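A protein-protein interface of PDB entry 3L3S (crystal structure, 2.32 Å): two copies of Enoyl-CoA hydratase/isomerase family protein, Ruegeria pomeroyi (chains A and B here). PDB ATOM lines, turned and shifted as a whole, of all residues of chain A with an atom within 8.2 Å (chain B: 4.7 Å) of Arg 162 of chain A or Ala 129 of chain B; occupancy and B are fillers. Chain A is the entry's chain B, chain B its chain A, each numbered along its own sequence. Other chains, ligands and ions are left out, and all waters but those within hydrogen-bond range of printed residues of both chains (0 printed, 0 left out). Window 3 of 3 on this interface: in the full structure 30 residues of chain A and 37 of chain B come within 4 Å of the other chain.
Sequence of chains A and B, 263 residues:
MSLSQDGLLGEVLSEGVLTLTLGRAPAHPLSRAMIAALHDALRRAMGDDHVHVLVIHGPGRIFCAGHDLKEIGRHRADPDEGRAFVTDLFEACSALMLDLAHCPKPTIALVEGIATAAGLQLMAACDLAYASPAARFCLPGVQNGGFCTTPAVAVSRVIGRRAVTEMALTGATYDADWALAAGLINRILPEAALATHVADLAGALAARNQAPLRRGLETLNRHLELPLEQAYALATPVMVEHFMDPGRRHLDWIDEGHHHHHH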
ATOM      1  N   ILE A 159       7.365  11.863 -12.521  1.00  0.00           N
ATOM      2  CA  ILE A 159       6.243  12.185 -11.618  1.00  0.00           C
ATOM      3  C   ILE A 159       6.521  11.578 -10.244  1.00  0.00           C
ATOM      4  O   ILE A 159       7.355  10.685 -10.125  1.00  0.00           O
ATOM      5  CB  ILE A 159       4.818  11.741 -12.154  1.00  0.00           C
ATOM      6  CG1 ILE A 159       4.723  10.232 -12.386  1.00  0.00           C
ATOM      7  CG2 ILE A 159       4.466  12.477 -13.422  1.00  0.00           C
ATOM      8  CD1 ILE A 159       3.345   9.762 -12.839  1.00  0.00           C
ATOM      9  N   GLY A 160       5.799  12.042  -9.222  1.00  0.00           N
ATOM     10  CA  GLY A 160       5.979  11.568  -7.850  1.00  0.00           C
ATOM     11  C   GLY A 160       5.641  10.106  -7.609  1.00  0.00           C
ATOM     12  O   GLY A 160       4.930   9.502  -8.416  1.00  0.00           O
ATOM     13  N   ARG A 161       6.123   9.552  -6.493  1.00  0.00           N
ATOM     14  CA  ARG A 161       5.894   8.146  -6.142  1.00  0.00           C
ATOM     15  C   ARG A 161       4.415   7.743  -5.998  1.00  0.00           C
ATOM     16  O   ARG A 161       4.061   6.611  -6.292  1.00  0.00           O
ATOM     17  CB  ARG A 161       6.689   7.763  -4.885  1.00  0.00           C
ATOM     18  CG  ARG A 161       6.797   6.257  -4.637  1.00  0.00           C
ATOM     19  CD  ARG A 161       7.438   5.938  -3.299  1.00  0.00           C
ATOM     20  NE  ARG A 161       8.898   6.022  -3.325  1.00  0.00           N
ATOM     21  CZ  ARG A 161       9.715   4.970  -3.273  1.00  0.00           C
ATOM     22  NH1 ARG A 161       9.233   3.729  -3.196  1.00  0.00           N
ATOM     23  NH2 ARG A 161      11.025   5.162  -3.282  1.00  0.00           N
ATOM     24  N   ARG A 162       3.561   8.676  -5.582  1.00  0.00           N
ATOM     25  CA  ARG A 162       2.133   8.401  -5.430  1.00  0.00           C
ATOM     26  C   ARG A 162       1.440   8.363  -6.780  1.00  0.00           C
ATOM     27  O   ARG A 162       0.569   7.525  -7.021  1.00  0.00           O
ATOM     28  CB  ARG A 162       1.462   9.472  -4.585  1.00  0.00           C
ATOM     29  CG  ARG A 162       1.883   9.479  -3.145  1.00  0.00           C
ATOM     30  CD  ARG A 162       1.166   8.464  -2.352  1.00  0.00           C
ATOM     31  NE  ARG A 162       1.176   8.779  -0.934  1.00  0.00           N
ATOM     32  CZ  ARG A 162       1.199   7.859   0.021  1.00  0.00           C
ATOM     33  NH1 ARG A 162       1.242   6.576  -0.300  1.00  0.00           N
ATOM     34  NH2 ARG A 162       1.079   8.219   1.288  1.00  0.00           N
ATOM     35  N   ALA A 163       1.871   9.265  -7.659  1.00  0.00           N
ATOM     36  CA  ALA A 163       1.320   9.398  -8.993  1.00  0.00           C
ATOM     37  C   ALA A 163       1.545   8.169  -9.870  1.00  0.00           C
ATOM     38  O   ALA A 163       0.579   7.632 -10.409  1.00  0.00           O
ATOM     39  CB  ALA A 163       1.857  10.642  -9.639  1.00  0.00           C
ATOM     40  N   VAL A 164       2.790   7.673  -9.931  1.00  0.00           N
ATOM     41  CA  VAL A 164       3.129   6.476 -10.727  1.00  0.00           C
ATOM     42  C   VAL A 164       2.493   5.220 -10.165  1.00  0.00           C
ATOM     43  O   VAL A 164       2.161   4.307 -10.914  1.00  0.00           O
ATOM     44  CB  VAL A 164       4.635   6.132 -10.754  1.00  0.00           C
ATOM     45  CG1 VAL A 164       5.025   5.620 -12.126  1.00  0.00           C
ATOM     46  CG2 VAL A 164       5.486   7.259 -10.284  1.00  0.00           C
ATOM     47  N   THR A 165       2.395   5.156  -8.838  1.00  0.00           N
ATOM     48  CA  THR A 165       1.807   4.008  -8.171  1.00  0.00           C
ATOM     49  C   THR A 165       0.312   3.914  -8.466  1.00  0.00           C
ATOM     50  O   THR A 165      -0.191   2.816  -8.671  1.00  0.00           O
ATOM     51  CB  THR A 165       2.097   4.010  -6.654  1.00  0.00           C
ATOM     52  OG1 THR A 165       3.515   4.096  -6.456  1.00  0.00           O
ATOM     53  CG2 THR A 165       1.615   2.712  -5.994  1.00  0.00           C
ATOM     54  N   GLU A 166      -0.364   5.057  -8.587  1.00  0.00           N
ATOM     55  CA  GLU A 166      -1.786   5.039  -8.887  1.00  0.00           C
ATOM     56  C   GLU A 166      -2.046   4.686 -10.348  1.00  0.00           C
ATOM     57  O   GLU A 166      -2.970   3.933 -10.630  1.00  0.00           O
ATOM     58  CB  GLU A 166      -2.488   6.347  -8.503  1.00  0.00           C
ATOM     59  CG  GLU A 166      -4.010   6.147  -8.286  1.00  0.00           C
ATOM     60  CD  GLU A 166      -4.817   7.437  -8.258  1.00  0.00           C
ATOM     61  OE1 GLU A 166      -4.609   8.311  -9.129  1.00  0.00           O
ATOM     62  OE2 GLU A 166      -5.680   7.564  -7.366  1.00  0.00           O
ATOM     63  N   MET A 167      -1.180   5.151 -11.254  1.00  0.00           N
ATOM     64  CA  MET A 167      -1.323   4.871 -12.683  1.00  0.00           C
ATOM     65  C   MET A 167      -1.142   3.392 -12.970  1.00  0.00           C
ATOM     66  O   MET A 167      -1.984   2.769 -13.619  1.00  0.00           O
ATOM     67  CB  MET A 167      -0.304   5.643 -13.526  1.00  0.00           C
ATOM     68  CG  MET A 167      -0.401   7.130 -13.491  1.00  0.00           C
ATOM     69  SD  MET A 167       0.667   7.881 -14.932  1.00  0.00           S
ATOM     70  CE  MET A 167      -0.651   7.769 -16.360  1.00  0.00           C
ATOM     71  N   ALA A 168      -0.058   2.839 -12.433  1.00  0.00           N
ATOM     72  CA  ALA A 168       0.304   1.440 -12.613  1.00  0.00           C
ATOM     73  C   ALA A 168      -0.676   0.454 -11.985  1.00  0.00           C
ATOM     74  O   ALA A 168      -1.022  -0.541 -12.612  1.00  0.00           O
ATOM     75  CB  ALA A 168       1.700   1.208 -12.096  1.00  0.00           C
ATOM     76  N   LEU A 169      -1.156   0.757 -10.778  1.00  0.00           N
ATOM     77  CA  LEU A 169      -2.104  -0.112 -10.076  1.00  0.00           C
ATOM     78  C   LEU A 169      -3.551  -0.072 -10.580  1.00  0.00           C
ATOM     79  O   LEU A 169      -4.167  -1.131 -10.732  1.00  0.00           O
ATOM     80  CB  LEU A 169      -2.083   0.137  -8.565  1.00  0.00           C
ATOM     81  CG  LEU A 169      -0.846  -0.198  -7.721  1.00  0.00           C
ATOM     82  CD1 LEU A 169      -1.199   0.005  -6.256  1.00  0.00           C
ATOM     83  CD2 LEU A 169      -0.361  -1.610  -7.950  1.00  0.00           C
ATOM     84  N   TYR A 174      -5.783   9.332 -17.500  1.00  0.00           N
ATOM     85  CA  TYR A 174      -5.678  10.638 -16.864  1.00  0.00           C
ATOM     86  C   TYR A 174      -5.604  11.714 -17.923  1.00  0.00           C
ATOM     87  O   TYR A 174      -4.966  11.511 -18.953  1.00  0.00           O
ATOM     88  CB  TYR A 174      -4.424  10.679 -15.997  1.00  0.00           C
ATOM     89  CG  TYR A 174      -4.452   9.726 -14.819  1.00  0.00           C
ATOM     90  CD1 TYR A 174      -4.909  10.154 -13.555  1.00  0.00           C
ATOM     91  CD2 TYR A 174      -4.014   8.395 -14.954  1.00  0.00           C
ATOM     92  CE1 TYR A 174      -4.924   9.279 -12.445  1.00  0.00           C
ATOM     93  CE2 TYR A 174      -4.028   7.510 -13.854  1.00  0.00           C
ATOM     94  CZ  TYR A 174      -4.483   7.965 -12.607  1.00  0.00           C
ATOM     95  OH  TYR A 174      -4.498   7.117 -11.540  1.00  0.00           O
ATOM     96  N   TRP A 178      -4.111  16.861 -15.142  1.00  0.00           N
ATOM     97  CA  TRP A 178      -3.512  16.043 -14.084  1.00  0.00           C
ATOM     98  C   TRP A 178      -2.037  15.873 -14.413  1.00  0.00           C
ATOM     99  O   TRP A 178      -1.197  15.906 -13.524  1.00  0.00           O
ATOM    100  CB  TRP A 178      -4.204  14.666 -14.011  1.00  0.00           C
ATOM    101  CG  TRP A 178      -3.733  13.737 -12.903  1.00  0.00           C
ATOM    102  CD1 TRP A 178      -4.258  13.633 -11.643  1.00  0.00           C
ATOM    103  CD2 TRP A 178      -2.653  12.793 -12.965  1.00  0.00           C
ATOM    104  NE1 TRP A 178      -3.572  12.687 -10.917  1.00  0.00           N
ATOM    105  CE2 TRP A 178      -2.582  12.155 -11.699  1.00  0.00           C
ATOM    106  CE3 TRP A 178      -1.733  12.418 -13.971  1.00  0.00           C
ATOM    107  CZ2 TRP A 178      -1.621  11.155 -11.406  1.00  0.00           C
ATOM    108  CZ3 TRP A 178      -0.772  11.423 -13.684  1.00  0.00           C
ATOM    109  CH2 TRP A 178      -0.728  10.805 -12.407  1.00  0.00           C
ATOM    110  N   ALA B 109      -4.414   3.452   2.175  1.00  0.00           N
ATOM    111  CA  ALA B 109      -4.750   4.159   3.400  1.00  0.00           C
ATOM    112  C   ALA B 109      -6.036   4.969   3.220  1.00  0.00           C
ATOM    113  O   ALA B 109      -6.158   5.757   2.277  1.00  0.00           O
ATOM    114  CB  ALA B 109      -3.610   5.060   3.828  1.00  0.00           C
ATOM    115  N   MET B 123       0.589   6.144   6.948  1.00  0.00           N
ATOM    116  CA  MET B 123      -0.161   6.543   5.771  1.00  0.00           C
ATOM    117  C   MET B 123       0.818   6.639   4.587  1.00  0.00           C
ATOM    118  O   MET B 123       0.551   6.115   3.505  1.00  0.00           O
ATOM    119  CB  MET B 123      -0.799   7.911   6.037  1.00  0.00           C
ATOM    120  CG  MET B 123      -1.872   8.301   5.058  1.00  0.00           C
ATOM    121  SD  MET B 123      -1.890  10.209   4.713  1.00  0.00           S
ATOM    122  CE  MET B 123      -0.242  10.227   3.689  1.00  0.00           C
ATOM    123  N   ALA B 124       1.978   7.247   4.843  1.00  0.00           N
ATOM    124  CA  ALA B 124       3.030   7.446   3.836  1.00  0.00           C
ATOM    125  C   ALA B 124       3.650   6.150   3.312  1.00  0.00           C
ATOM    126  O   ALA B 124       3.910   6.028   2.110  1.00  0.00           O
ATOM    127  CB  ALA B 124       4.109   8.373   4.378  1.00  0.00           C
ATOM    128  N   CYS B 126       2.151   3.402   2.955  1.00  0.00           N
ATOM    129  CA  CYS B 126       1.170   2.712   2.111  1.00  0.00           C
ATOM    130  C   CYS B 126       1.405   3.082   0.642  1.00  0.00           C
ATOM    131  O   CYS B 126       1.900   4.170   0.347  1.00  0.00           O
ATOM    132  CB  CYS B 126      -0.272   3.068   2.518  1.00  0.00           C
ATOM    133  SG  CYS B 126      -0.782   2.487   4.153  1.00  0.00           S
ATOM    134  N   ASP B 127       1.071   2.169  -0.267  1.00  0.00           N
ATOM    135  CA  ASP B 127       1.245   2.402  -1.704  1.00  0.00           C
ATOM    136  C   ASP B 127       0.341   3.521  -2.212  1.00  0.00           C
ATOM    137  O   ASP B 127       0.727   4.295  -3.091  1.00  0.00           O
ATOM    138  CB  ASP B 127       0.968   1.124  -2.493  1.00  0.00           C
ATOM    139  CG  ASP B 127       1.987   0.031  -2.221  1.00  0.00           C
ATOM    140  OD1 ASP B 127       3.188   0.255  -2.473  1.00  0.00           O
ATOM    141  OD2 ASP B 127       1.585  -1.060  -1.764  1.00  0.00           O
ATOM    142  N   LEU B 128      -0.864   3.596  -1.646  1.00  0.00           N
ATOM    143  CA  LEU B 128      -1.866   4.600  -2.005  1.00  0.00           C
ATOM    144  C   LEU B 128      -2.501   5.218  -0.764  1.00  0.00           C
ATOM    145  O   LEU B 128      -2.407   4.664   0.334  1.00  0.00           O
ATOM    146  CB  LEU B 128      -2.978   3.992  -2.890  1.00  0.00           C
ATOM    147  CG  LEU B 128      -2.623   3.361  -4.245  1.00  0.00           C
ATOM    148  CD1 LEU B 128      -3.842   2.792  -4.952  1.00  0.00           C
ATOM    149  CD2 LEU B 128      -1.919   4.393  -5.109  1.00  0.00           C
ATOM    150  N   ALA B 129      -3.120   6.382  -0.941  1.00  0.00           N
ATOM    151  CA  ALA B 129      -3.786   7.079   0.160  1.00  0.00           C
ATOM    152  C   ALA B 129      -4.925   7.958  -0.335  1.00  0.00           C
ATOM    153  O   ALA B 129      -4.748   8.771  -1.254  1.00  0.00           O
ATOM    154  CB  ALA B 129      -2.781   7.917   0.984  1.00  0.00           C
ATOM    155  N   TYR B 130      -6.100   7.772   0.268  1.00  0.00           N
ATOM    156  CA  TYR B 130      -7.292   8.549  -0.079  1.00  0.00           C
ATOM    157  C   TYR B 130      -7.840   9.273   1.142  1.00  0.00           C
ATOM    158  O   TYR B 130      -7.871   8.717   2.245  1.00  0.00           O
ATOM    159  CB  TYR B 130      -8.353   7.650  -0.715  1.00  0.00           C
ATOM    160  CG  TYR B 130      -7.878   7.029  -2.006  1.00  0.00           C
ATOM    161  CD1 TYR B 130      -7.730   7.815  -3.172  1.00  0.00           C
ATOM    162  CD2 TYR B 130      -7.471   5.682  -2.050  1.00  0.00           C
ATOM    163  CE1 TYR B 130      -7.177   7.269  -4.353  1.00  0.00           C
ATOM    164  CE2 TYR B 130      -6.911   5.124  -3.226  1.00  0.00           C
ATOM    165  CZ  TYR B 130      -6.768   5.930  -4.369  1.00  0.00           C
ATOM    166  OH  TYR B 130      -6.205   5.411  -5.507  1.00  0.00           O
ATOM    167  N   ALA B 131      -8.253  10.520   0.942  1.00  0.00           N
ATOM    168  CA  ALA B 131      -8.765  11.317   2.032  1.00  0.00           C
ATOM    169  C   ALA B 131     -10.021  12.106   1.758  1.00  0.00           C
ATOM    170  O   ALA B 131     -10.478  12.217   0.622  1.00  0.00           O
ATOM    171  CB  ALA B 131      -7.685  12.232   2.559  1.00  0.00           C
ATOM    172  N   VAL B 158       7.522  10.432  -0.445  1.00  0.00           N
ATOM    173  CA  VAL B 158       6.204  10.686  -1.017  1.00  0.00           C
ATOM    174  C   VAL B 158       5.931  12.153  -1.425  1.00  0.00           C
ATOM    175  O   VAL B 158       5.048  12.407  -2.257  1.00  0.00           O
ATOM    176  CB  VAL B 158       5.131  10.028  -0.090  1.00  0.00           C
ATOM    177  CG1 VAL B 158       3.852  10.806  -0.015  1.00  0.00           C
ATOM    178  CG2 VAL B 158       4.865   8.601  -0.576  1.00  0.00           C
ATOM    179  N   GLY B 183       1.459  15.699  -3.176  1.00  0.00           N
ATOM    180  CA  GLY B 183       1.514  14.287  -3.515  1.00  0.00           C
ATOM    181  C   GLY B 183       1.510  13.373  -2.301  1.00  0.00           C
ATOM    182  O   GLY B 183       2.013  12.273  -2.376  1.00  0.00           O
ATOM    183  N   LEU B 184       0.988  13.853  -1.175  1.00  0.00           N
ATOM    184  CA  LEU B 184       0.895  13.088   0.069  1.00  0.00           C
ATOM    185  C   LEU B 184      -0.286  12.122  -0.016  1.00  0.00           C
ATOM    186  O   LEU B 184      -0.246  11.019   0.542  1.00  0.00           O
ATOM    187  CB  LEU B 184       0.765  14.051   1.248  1.00  0.00           C
ATOM    188  CG  LEU B 184       0.967  13.714   2.719  1.00  0.00           C
ATOM    189  CD1 LEU B 184       2.263  12.975   2.962  1.00  0.00           C
ATOM    190  CD2 LEU B 184       0.960  15.016   3.488  1.00  0.00           C
ATOM    191  N   ILE B 185      -1.344  12.570  -0.687  1.00  0.00           N
ATOM    192  CA  ILE B 185      -2.526  11.741  -0.928  1.00  0.00           C
ATOM    193  C   ILE B 185      -2.777  11.703  -2.435  1.00  0.00           C
ATOM    194  O   ILE B 185      -2.355  12.615  -3.158  1.00  0.00           O
ATOM    195  CB  ILE B 185      -3.797  12.207  -0.144  1.00  0.00           C
ATOM    196  CG1 ILE B 185      -3.964  13.727  -0.202  1.00  0.00           C
ATOM    197  CG2 ILE B 185      -3.745  11.683   1.293  1.00  0.00           C
ATOM    198  CD1 ILE B 185      -5.276  14.272   0.335  1.00  0.00           C
ATOM    199  N   ASN B 186      -3.383  10.612  -2.902  1.00  0.00           N
ATOM    200  CA  ASN B 186      -3.684  10.423  -4.326  1.00  0.00           C
ATOM    201  C   ASN B 186      -4.865  11.238  -4.855  1.00  0.00           C
ATOM    202  O   ASN B 186      -4.736  11.876  -5.890  1.00  0.00           O
ATOM    203  CB  ASN B 186      -3.889   8.939  -4.656  1.00  0.00           C
ATOM    204  CG  ASN B 186      -2.620   8.123  -4.512  1.00  0.00           C
ATOM    205  OD1 ASN B 186      -2.352   7.557  -3.455  1.00  0.00           O
ATOM    206  ND2 ASN B 186      -1.835   8.055  -5.578  1.00  0.00           N
ATOM    207  N   ARG B 187      -6.011  11.189  -4.168  1.00  0.00           N
ATOM    208  CA  ARG B 187      -7.241  11.922  -4.554  1.00  0.00           C
ATOM    209  C   ARG B 187      -8.088  12.316  -3.333  1.00  0.00           C
ATOM    210  O   ARG B 187      -8.061  11.637  -2.307  1.00  0.00           O
ATOM    211  CB  ARG B 187      -8.129  11.084  -5.508  1.00  0.00           C
ATOM    212  CG  ARG B 187      -7.680  10.993  -6.975  1.00  0.00           C
ATOM    213  CD  ARG B 187      -8.531  10.006  -7.766  1.00  0.00           C
ATOM    214  NE  ARG B 187      -7.872   9.568  -9.002  1.00  0.00           N
ATOM    215  CZ  ARG B 187      -8.393   8.710  -9.880  1.00  0.00           C
ATOM    216  NH1 ARG B 187      -9.596   8.184  -9.681  1.00  0.00           N
ATOM    217  NH2 ARG B 187      -7.694   8.346 -10.945  1.00  0.00           N
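The backbone carbonyl oxygen (O) of Met 123 of chain B sits at hydrogen-bond distance from the guanidinium group (NH2) of Arg 162 of chain A. The backbone carbonyl oxygen (O) of Cys 126 of chain B is in hydrogen-bond range of the guanidinium group (NH1) of Arg 162 of chain A. The side-chain hydroxyl (OH) of Tyr 130 of chain B sits at hydrogen-bond distance from the side-chain carboxylate (OE2) of Glu 166 of chain A, at 2.9 Å. The guanidinium group of Arg 162 of chain A is in hydrogen-bond range of the backbone carbonyl oxygen of Leu 184 of chain B. ND2 of Asn 186 of chain B is in hydrogen-bond range of O of Arg 162 of chain A, at 2.9 Å. OE2 of Glu 166 of chain A lies within salt-bridge range of NE of Arg 187 of chain B (3.4 Å). The side-chain hydroxyl (OH) of Tyr 174 of chain A lies close to the guanidinium group (NH2) of Arg 187 of chain B (3.5 Å).
N of Ala 109 of chain B is in hydrogen-bond range of O of Leu 128 of chain B (3.0 Å). N of Tyr 130 of chain B sits at hydrogen-bond distance from O of Ala 109 of chain B, at 2.8 Å. The backbone carbonyl oxygen (O) of Ala 129 of chain B sits at hydrogen-bond distance from the backbone NH (N) of Asn 186 of chain B (2.8 Å). The backbone NH (N) of Ala 131 of chain B sits at hydrogen-bond distance from the backbone carbonyl oxygen (O) of Arg 187 of chain B, at 3.4 Å. The backbone carbonyl oxygen (O) of Arg 161 of chain A sits at hydrogen-bond distance from the side-chain hydroxyl (OG1) of Thr 165 of chain A (2.6 Å). The side-chain carboxylate (OE1) of Glu 166 of chain A is in hydrogen-bond range of the side-chain hydroxyl (OH) of Tyr 174 of chain A, 2.7 Å away.
NH2 of Arg 162 of chain A touches CA of Ala 124 of chain B (3.3 Å). Arg 162 of chain A touches Asp 127 of chain B. NH1 of Arg 162 of chain A touches N of Leu 128 of chain B, 3.9 Å away. Ala 129 of chain B touches Arg 162 of chain A (CB to NH2, 3.9 Å). Arg 162 of chain A touches Val 158 of chain B. CG of Arg 162 of chain A touches O of Gly 183 of chain B, 2.9 Å away. Thr 165 of chain A touches Asp 127 of chain B (CG2 to O, 3.4 Å). CD2 of Leu 128 of chain B touches CA of Glu 166 of chain A, at 3.8 Å. Glu 166 of chain A touches Asn 186 of chain B (CB to ND2, 3.4 Å).
Gly 160 of chain A touches none of the printed residues of chain B. Arg 162 of chain A touches just these residues of chain B: Met 123, Ala 124, Cys 126, Asp 127, Leu 128, Ala 129, Val 158, Gly 183, Leu 184 and Asn 186. Printed residues of chain A within 4 Å of Cys 126 of chain B: Arg 162 (2.6 Å). Of chain A, only Arg 162 (3.9 Å) comes within 4 Å of Ala 129 of chain B. Of the printed residues of chain A, Tyr 130 of chain B touches Glu 166. Printed residues of chain A within 4 Å of Gly 183 of chain B: Arg 162 (2.9 Å). The nearest printed residue of chain A that does not touch Leu 128 of chain B is Thr 165 of chain A (4.01 Å).
Among the printed residues, Asp or Glu carboxylates within 4 Å of a Lys or Arg side-chain nitrogen of the other chain: Glu 166 of chain A with Arg 187 of chain B (3.4 Å).
No position is printed for both chains. Of the 16 pairs that touch across the chains among the printed residues, none has its exchanged pair printed and touching as well.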
